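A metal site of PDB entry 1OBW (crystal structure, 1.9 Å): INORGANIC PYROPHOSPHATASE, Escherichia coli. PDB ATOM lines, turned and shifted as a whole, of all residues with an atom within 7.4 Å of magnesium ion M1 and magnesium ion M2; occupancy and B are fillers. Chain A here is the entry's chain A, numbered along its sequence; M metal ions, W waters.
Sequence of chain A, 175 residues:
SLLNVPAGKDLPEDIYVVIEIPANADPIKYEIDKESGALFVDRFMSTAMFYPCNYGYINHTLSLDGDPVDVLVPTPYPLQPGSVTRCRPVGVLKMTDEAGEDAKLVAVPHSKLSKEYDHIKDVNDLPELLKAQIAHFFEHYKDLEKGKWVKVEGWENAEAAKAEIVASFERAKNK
NZ of Lys 104 is in salt-bridge range of OD2 of Asp 102 (3.3 Å). The side-chain carboxylate of Asp 102 sits close to the side-chain carboxylate of Asp 97. The side-chain hydroxyl (OG) of Ser 63 sits at hydrogen-bond distance from the side-chain carboxylate (OD1) of Asp 65, 2.6 Å away. The backbone NH of Asp 67 is in hydrogen-bond range of the side-chain carboxylate of Asp 65, at 3.0 Å. The side-chain carboxylate of Asp 70 lies close to the side-chain amino group of Lys 104, 2.8 Å away. The side-chain carboxylate (OD2) of Asp 70 sits close to the side-chain hydroxyl (OH) of Tyr 55, at 3.3 Å. The side-chain amino group (NZ) of Lys 104 lies within hydrogen-bond range of the side-chain hydroxyl (OH) of Tyr 55.
Magnesium ion M1 is bound by OD1 of Asp 102 (2.0 Å), OD2 of Asp 65 (2.0 Å), water W5 (2.0 Å), water W2 (2.1 Å), water W8 (2.2 Å) and OD2 of Asp 70 (2.2 Å). Magnesium ion M1 has six donor atoms within binding distance.
Water W1 bridges the side-chain carboxylate (OE1) of Glu 20 and the backbone carbonyl oxygen (O) of Gly 56.
Water W4 is bound to magnesium ion M2, 2.0 Å away. Water W7 binds magnesium ion M2 (2.0 Å). Magnesium ion M2 is bound by OD1 of Asp 70 (2.1 Å). Magnesium ion M2 is bound by water W1, 2.1 Å away. Water W3 is bound to magnesium ion M2, 2.2 Å away. Magnesium ion M2 has five donor atoms within binding distance. Slightly farther from magnesium ion M2 lies water W6 (2.7 Å).
Merely in contact with magnesium ion M1: Lys 104. Of the 25 residues printed, 4 come within 4 Å of magnesium ion M1.
Within 4 Å of magnesium ion M2: Asp 70.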
ATOM      1  N   GLU A  20      22.079  25.856  30.413  1.00  0.00           N
ATOM      2  CA  GLU A  20      20.855  26.627  30.543  1.00  0.00           C
ATOM      3  C   GLU A  20      20.765  27.448  31.833  1.00  0.00           C
ATOM      4  O   GLU A  20      20.127  28.504  31.782  1.00  0.00           O
ATOM      5  CB  GLU A  20      19.627  25.628  30.545  1.00  0.00           C
ATOM      6  CG  GLU A  20      19.649  25.040  29.072  1.00  0.00           C
ATOM      7  CD  GLU A  20      18.589  23.931  29.050  1.00  0.00           C
ATOM      8  OE1 GLU A  20      18.643  23.065  29.925  1.00  0.00           O
ATOM      9  OE2 GLU A  20      17.704  23.956  28.177  1.00  0.00           O
ATOM     10  N   LYS A  29      14.007  28.726  36.034  1.00  0.00           N
ATOM     11  CA  LYS A  29      14.316  27.627  35.141  1.00  0.00           C
ATOM     12  C   LYS A  29      14.275  28.105  33.699  1.00  0.00           C
ATOM     13  O   LYS A  29      13.208  28.427  33.195  1.00  0.00           O
ATOM     14  CB  LYS A  29      13.292  26.499  35.333  1.00  0.00           C
ATOM     15  CG  LYS A  29      13.738  25.169  34.707  1.00  0.00           C
ATOM     16  CD  LYS A  29      12.631  24.166  35.084  1.00  0.00           C
ATOM     17  CE  LYS A  29      12.992  22.785  34.532  1.00  0.00           C
ATOM     18  NZ  LYS A  29      12.527  22.661  33.115  1.00  0.00           N
ATOM     19  N   TYR A  30      15.430  28.148  33.045  1.00  0.00           N
ATOM     20  CA  TYR A  30      15.488  28.541  31.647  1.00  0.00           C
ATOM     21  C   TYR A  30      15.600  27.236  30.833  1.00  0.00           C
ATOM     22  O   TYR A  30      16.096  26.252  31.354  1.00  0.00           O
ATOM     23  CB  TYR A  30      16.753  29.355  31.369  1.00  0.00           C
ATOM     24  CG  TYR A  30      16.733  30.769  31.961  1.00  0.00           C
ATOM     25  CD1 TYR A  30      15.977  31.767  31.341  1.00  0.00           C
ATOM     26  CD2 TYR A  30      17.475  31.114  33.077  1.00  0.00           C
ATOM     27  CE1 TYR A  30      16.019  33.066  31.821  1.00  0.00           C
ATOM     28  CE2 TYR A  30      17.503  32.392  33.578  1.00  0.00           C
ATOM     29  CZ  TYR A  30      16.747  33.371  32.943  1.00  0.00           C
ATOM     30  OH  TYR A  30      16.705  34.685  33.390  1.00  0.00           O
ATOM     31  N   GLU A  31      15.182  27.310  29.588  1.00  0.00           N
ATOM     32  CA  GLU A  31      15.396  26.243  28.626  1.00  0.00           C
ATOM     33  C   GLU A  31      15.775  26.822  27.262  1.00  0.00           C
ATOM     34  O   GLU A  31      15.267  27.891  26.887  1.00  0.00           O
ATOM     35  CB  GLU A  31      14.062  25.484  28.577  1.00  0.00           C
ATOM     36  CG  GLU A  31      14.079  24.316  27.638  1.00  0.00           C
ATOM     37  CD  GLU A  31      12.748  23.577  27.550  1.00  0.00           C
ATOM     38  OE1 GLU A  31      11.809  23.929  28.294  1.00  0.00           O
ATOM     39  OE2 GLU A  31      12.707  22.641  26.704  1.00  0.00           O
ATOM     40  N   LYS A  34      14.269  24.705  21.069  1.00  0.00           N
ATOM     41  CA  LYS A  34      14.648  24.004  19.851  1.00  0.00           C
ATOM     42  C   LYS A  34      14.390  24.688  18.516  1.00  0.00           C
ATOM     43  O   LYS A  34      15.258  24.659  17.645  1.00  0.00           O
ATOM     44  CB  LYS A  34      13.934  22.644  19.897  1.00  0.00           C
ATOM     45  CG  LYS A  34      14.651  21.644  20.802  1.00  0.00           C
ATOM     46  CD  LYS A  34      14.021  21.617  22.195  1.00  0.00           C
ATOM     47  CE  LYS A  34      14.486  20.403  22.989  1.00  0.00           C
ATOM     48  NZ  LYS A  34      13.322  19.530  23.343  1.00  0.00           N
ATOM     49  N   TYR A  55      23.441  23.611  34.981  1.00  0.00           N
ATOM     50  CA  TYR A  55      22.514  22.617  34.461  1.00  0.00           C
ATOM     51  C   TYR A  55      22.361  22.861  32.956  1.00  0.00           C
ATOM     52  O   TYR A  55      22.264  24.009  32.539  1.00  0.00           O
ATOM     53  CB  TYR A  55      21.141  22.755  35.135  1.00  0.00           C
ATOM     54  CG  TYR A  55      20.105  21.730  34.730  1.00  0.00           C
ATOM     55  CD1 TYR A  55      20.221  20.407  35.127  1.00  0.00           C
ATOM     56  CD2 TYR A  55      19.013  22.084  33.942  1.00  0.00           C
ATOM     57  CE1 TYR A  55      19.262  19.449  34.761  1.00  0.00           C
ATOM     58  CE2 TYR A  55      18.056  21.148  33.568  1.00  0.00           C
ATOM     59  CZ  TYR A  55      18.182  19.842  33.990  1.00  0.00           C
ATOM     60  OH  TYR A  55      17.242  18.895  33.617  1.00  0.00           O
ATOM     61  N   GLY A  56      22.418  21.803  32.155  1.00  0.00           N
ATOM     62  CA  GLY A  56      22.066  21.968  30.752  1.00  0.00           C
ATOM     63  C   GLY A  56      21.832  20.612  30.024  1.00  0.00           C
ATOM     64  O   GLY A  56      21.304  19.729  30.649  1.00  0.00           O
ATOM     65  N   TYR A  57      22.277  20.601  28.759  1.00  0.00           N
ATOM     66  CA  TYR A  57      21.959  19.406  27.981  1.00  0.00           C
ATOM     67  C   TYR A  57      23.038  19.137  26.941  1.00  0.00           C
ATOM     68  O   TYR A  57      23.911  19.952  26.654  1.00  0.00           O
ATOM     69  CB  TYR A  57      20.589  19.503  27.292  1.00  0.00           C
ATOM     70  CG  TYR A  57      20.579  20.571  26.215  1.00  0.00           C
ATOM     71  CD1 TYR A  57      20.366  21.877  26.619  1.00  0.00           C
ATOM     72  CD2 TYR A  57      20.761  20.313  24.863  1.00  0.00           C
ATOM     73  CE1 TYR A  57      20.365  22.915  25.721  1.00  0.00           C
ATOM     74  CE2 TYR A  57      20.746  21.328  23.921  1.00  0.00           C
ATOM     75  CZ  TYR A  57      20.537  22.641  24.375  1.00  0.00           C
ATOM     76  OH  TYR A  57      20.511  23.701  23.517  1.00  0.00           O
ATOM     77  N   ILE A  58      22.956  17.918  26.377  1.00  0.00           N
ATOM     78  CA  ILE A  58      23.860  17.560  25.278  1.00  0.00           C
ATOM     79  C   ILE A  58      23.057  17.640  23.957  1.00  0.00           C
ATOM     80  O   ILE A  58      22.040  16.978  23.822  1.00  0.00           O
ATOM     81  CB  ILE A  58      24.362  16.111  25.364  1.00  0.00           C
ATOM     82  CG1 ILE A  58      25.084  15.851  26.706  1.00  0.00           C
ATOM     83  CG2 ILE A  58      25.327  15.843  24.215  1.00  0.00           C
ATOM     84  CD1 ILE A  58      25.649  14.472  26.929  1.00  0.00           C
ATOM     85  N   SER A  63      16.631  11.630  24.861  1.00  0.00           N
ATOM     86  CA  SER A  63      16.568  10.633  25.927  1.00  0.00           C
ATOM     87  C   SER A  63      15.191   9.975  25.926  1.00  0.00           C
ATOM     88  O   SER A  63      14.325  10.349  25.146  1.00  0.00           O
ATOM     89  CB  SER A  63      16.820  11.289  27.299  1.00  0.00           C
ATOM     90  OG  SER A  63      15.626  11.974  27.656  1.00  0.00           O
ATOM     91  N   LEU A  64      14.936   9.078  26.873  1.00  0.00           N
ATOM     92  CA  LEU A  64      13.649   8.405  27.001  1.00  0.00           C
ATOM     93  C   LEU A  64      12.525   9.365  27.361  1.00  0.00           C
ATOM     94  O   LEU A  64      11.362   9.043  27.139  1.00  0.00           O
ATOM     95  CB  LEU A  64      13.712   7.364  28.102  1.00  0.00           C
ATOM     96  CG  LEU A  64      13.894   5.864  27.939  1.00  0.00           C
ATOM     97  CD1 LEU A  64      13.879   5.403  26.494  1.00  0.00           C
ATOM     98  CD2 LEU A  64      15.162   5.410  28.677  1.00  0.00           C
ATOM     99  N   ASP A  65      12.808  10.563  27.920  1.00  0.00           N
ATOM    100  CA  ASP A  65      11.752  11.464  28.310  1.00  0.00           C
ATOM    101  C   ASP A  65      11.321  12.376  27.173  1.00  0.00           C
ATOM    102  O   ASP A  65      10.441  13.189  27.424  1.00  0.00           O
ATOM    103  CB  ASP A  65      12.055  12.320  29.544  1.00  0.00           C
ATOM    104  CG  ASP A  65      13.275  13.201  29.380  1.00  0.00           C
ATOM    105  OD1 ASP A  65      13.673  13.569  28.264  1.00  0.00           O
ATOM    106  OD2 ASP A  65      13.861  13.520  30.435  1.00  0.00           O
ATOM    107  N   GLY A  66      11.927  12.288  26.003  1.00  0.00           N
ATOM    108  CA  GLY A  66      11.536  13.114  24.878  1.00  0.00           C
ATOM    109  C   GLY A  66      12.390  14.347  24.669  1.00  0.00           C
ATOM    110  O   GLY A  66      12.150  15.105  23.733  1.00  0.00           O
ATOM    111  N   ASP A  67      13.460  14.565  25.443  1.00  0.00           N
ATOM    112  CA  ASP A  67      14.279  15.765  25.250  1.00  0.00           C
ATOM    113  C   ASP A  67      15.730  15.341  25.320  1.00  0.00           C
ATOM    114  O   ASP A  67      15.984  14.235  25.750  1.00  0.00           O
ATOM    115  CB  ASP A  67      14.141  16.761  26.426  1.00  0.00           C
ATOM    116  CG  ASP A  67      12.870  17.575  26.380  1.00  0.00           C
ATOM    117  OD1 ASP A  67      12.731  18.419  25.473  1.00  0.00           O
ATOM    118  OD2 ASP A  67      12.046  17.342  27.276  1.00  0.00           O
ATOM    119  N   PRO A  68      16.607  16.248  24.958  1.00  0.00           N
ATOM    120  CA  PRO A  68      18.045  15.973  25.055  1.00  0.00           C
ATOM    121  C   PRO A  68      18.388  15.519  26.460  1.00  0.00           C
ATOM    122  O   PRO A  68      17.725  15.947  27.442  1.00  0.00           O
ATOM    123  CB  PRO A  68      18.689  17.249  24.568  1.00  0.00           C
ATOM    124  CG  PRO A  68      17.640  17.924  23.731  1.00  0.00           C
ATOM    125  CD  PRO A  68      16.322  17.572  24.366  1.00  0.00           C
ATOM    126  N   VAL A  69      19.492  14.761  26.526  1.00  0.00           N
ATOM    127  CA  VAL A  69      20.000  14.257  27.803  1.00  0.00           C
ATOM    128  C   VAL A  69      20.282  15.481  28.737  1.00  0.00           C
ATOM    129  O   VAL A  69      20.976  16.357  28.289  1.00  0.00           O
ATOM    130  CB  VAL A  69      21.290  13.487  27.544  1.00  0.00           C
ATOM    131  CG1 VAL A  69      22.053  13.100  28.803  1.00  0.00           C
ATOM    132  CG2 VAL A  69      20.931  12.209  26.747  1.00  0.00           C
ATOM    133  N   ASP A  70      19.820  15.482  29.955  1.00  0.00           N
ATOM    134  CA  ASP A  70      20.113  16.575  30.899  1.00  0.00           C
ATOM    135  C   ASP A  70      21.398  16.279  31.678  1.00  0.00           C
ATOM    136  O   ASP A  70      21.732  15.122  31.995  1.00  0.00           O
ATOM    137  CB  ASP A  70      19.027  16.649  31.951  1.00  0.00           C
ATOM    138  CG  ASP A  70      17.631  16.898  31.366  1.00  0.00           C
ATOM    139  OD1 ASP A  70      17.471  17.770  30.518  1.00  0.00           O
ATOM    140  OD2 ASP A  70      16.721  16.223  31.826  1.00  0.00           O
ATOM    141  N   VAL A  71      22.203  17.307  31.972  1.00  0.00           N
ATOM    142  CA  VAL A  71      23.503  17.169  32.579  1.00  0.00           C
ATOM    143  C   VAL A  71      23.677  18.253  33.642  1.00  0.00           C
ATOM    144  O   VAL A  71      23.461  19.450  33.389  1.00  0.00           O
ATOM    145  CB  VAL A  71      24.630  17.325  31.530  1.00  0.00           C
ATOM    146  CG1 VAL A  71      25.991  16.928  32.106  1.00  0.00           C
ATOM    147  CG2 VAL A  71      24.381  16.460  30.269  1.00  0.00           C
ATOM    148  N   ASP A  97       9.662  10.974  36.626  1.00  0.00           N
ATOM    149  CA  ASP A  97       8.695  12.046  36.955  1.00  0.00           C
ATOM    150  C   ASP A  97       7.549  11.898  35.990  1.00  0.00           C
ATOM    151  O   ASP A  97       7.421  10.808  35.391  1.00  0.00           O
ATOM    152  CB  ASP A  97       9.403  13.402  36.975  1.00  0.00           C
ATOM    153  CG  ASP A  97      10.154  13.735  35.705  1.00  0.00           C
ATOM    154  OD1 ASP A  97       9.638  13.501  34.600  1.00  0.00           O
ATOM    155  OD2 ASP A  97      11.280  14.252  35.848  1.00  0.00           O
ATOM    156  N   ALA A  99       7.207  13.010  32.949  1.00  0.00           N
ATOM    157  CA  ALA A  99       7.698  12.842  31.601  1.00  0.00           C
ATOM    158  C   ALA A  99       8.243  11.448  31.267  1.00  0.00           C
ATOM    159  O   ALA A  99       8.597  11.157  30.099  1.00  0.00           O
ATOM    160  CB  ALA A  99       8.860  13.836  31.430  1.00  0.00           C
ATOM    161  N   GLU A 101      11.167   8.319  32.508  1.00  0.00           N
ATOM    162  CA  GLU A 101      12.513   8.286  33.073  1.00  0.00           C
ATOM    163  C   GLU A 101      13.246   9.556  32.648  1.00  0.00           C
ATOM    164  O   GLU A 101      13.434   9.873  31.477  1.00  0.00           O
ATOM    165  CB  GLU A 101      13.286   7.040  32.695  1.00  0.00           C
ATOM    166  CG  GLU A 101      14.749   6.975  33.134  1.00  0.00           C
ATOM    167  CD  GLU A 101      14.983   6.985  34.638  1.00  0.00           C
ATOM    168  OE1 GLU A 101      14.220   6.318  35.369  1.00  0.00           O
ATOM    169  OE2 GLU A 101      15.933   7.661  35.109  1.00  0.00           O
ATOM    170  N   ASP A 102      13.670  10.324  33.667  1.00  0.00           N
ATOM    171  CA  ASP A 102      14.278  11.633  33.400  1.00  0.00           C
ATOM    172  C   ASP A 102      15.621  11.735  34.123  1.00  0.00           C
ATOM    173  O   ASP A 102      15.785  12.451  35.149  1.00  0.00           O
ATOM    174  CB  ASP A 102      13.263  12.664  33.942  1.00  0.00           C
ATOM    175  CG  ASP A 102      13.708  14.086  33.600  1.00  0.00           C
ATOM    176  OD1 ASP A 102      14.721  14.331  32.902  1.00  0.00           O
ATOM    177  OD2 ASP A 102      12.989  14.980  34.075  1.00  0.00           O
ATOM    178  N   ALA A 103      16.616  11.009  33.632  1.00  0.00           N
ATOM    179  CA  ALA A 103      17.892  10.874  34.296  1.00  0.00           C
ATOM    180  C   ALA A 103      18.676  12.197  34.271  1.00  0.00           C
ATOM    181  O   ALA A 103      18.542  12.973  33.333  1.00  0.00           O
ATOM    182  CB  ALA A 103      18.772   9.778  33.722  1.00  0.00           C
ATOM    183  N   LYS A 104      19.436  12.438  35.355  1.00  0.00           N
ATOM    184  CA  LYS A 104      20.351  13.613  35.337  1.00  0.00           C
ATOM    185  C   LYS A 104      21.802  13.118  35.419  1.00  0.00           C
ATOM    186  O   LYS A 104      22.296  12.705  36.475  1.00  0.00           O
ATOM    187  CB  LYS A 104      20.016  14.580  36.470  1.00  0.00           C
ATOM    188  CG  LYS A 104      18.512  14.869  36.710  1.00  0.00           C
ATOM    189  CD  LYS A 104      17.902  15.667  35.567  1.00  0.00           C
ATOM    190  CE  LYS A 104      16.371  15.853  35.707  1.00  0.00           C
ATOM    191  NZ  LYS A 104      15.825  16.524  34.488  1.00  0.00           N
ATOM    192  N   GLU A 164      23.940   5.710  28.544  1.00  0.00           N
ATOM    193  CA  GLU A 164      22.785   6.576  28.269  1.00  0.00           C
ATOM    194  C   GLU A 164      23.175   7.580  27.189  1.00  0.00           C
ATOM    195  O   GLU A 164      22.333   7.914  26.356  1.00  0.00           O
ATOM    196  CB  GLU A 164      22.314   7.375  29.512  1.00  0.00           C
ATOM    197  CG  GLU A 164      21.054   8.169  29.204  1.00  0.00           C
ATOM    198  CD  GLU A 164      20.618   9.157  30.261  1.00  0.00           C
ATOM    199  OE1 GLU A 164      21.027   8.991  31.431  1.00  0.00           O
ATOM    200  OE2 GLU A 164      19.850  10.102  29.938  1.00  0.00           O
HETATM  201 MG    MG M   1      15.224  14.809  31.061  1.00  0.00          MG
HETATM  202 MG    MG M   2      16.586  19.331  29.498  1.00  0.00          MG
HETATM  203  O   HOH W   1      18.228  20.568  30.052  1.00  0.00           O
HETATM  204  O   HOH W   2      16.800  13.359  31.086  1.00  0.00           O
HETATM  205  O   HOH W   3      16.129  21.487  29.544  1.00  0.00           O
HETATM  206  O   HOH W   4      14.864  18.400  29.517  1.00  0.00           O
HETATM  207  O   HOH W   5      13.867  16.279  30.950  1.00  0.00           O
HETATM  208  O   HOH W   6      15.414  19.736  31.863  1.00  0.00           O
HETATM  209  O   HOH W   7      17.244  18.727  27.733  1.00  0.00           O
HETATM  210  O   HOH W   8      15.921  15.021  29.030  1.00  0.00           O
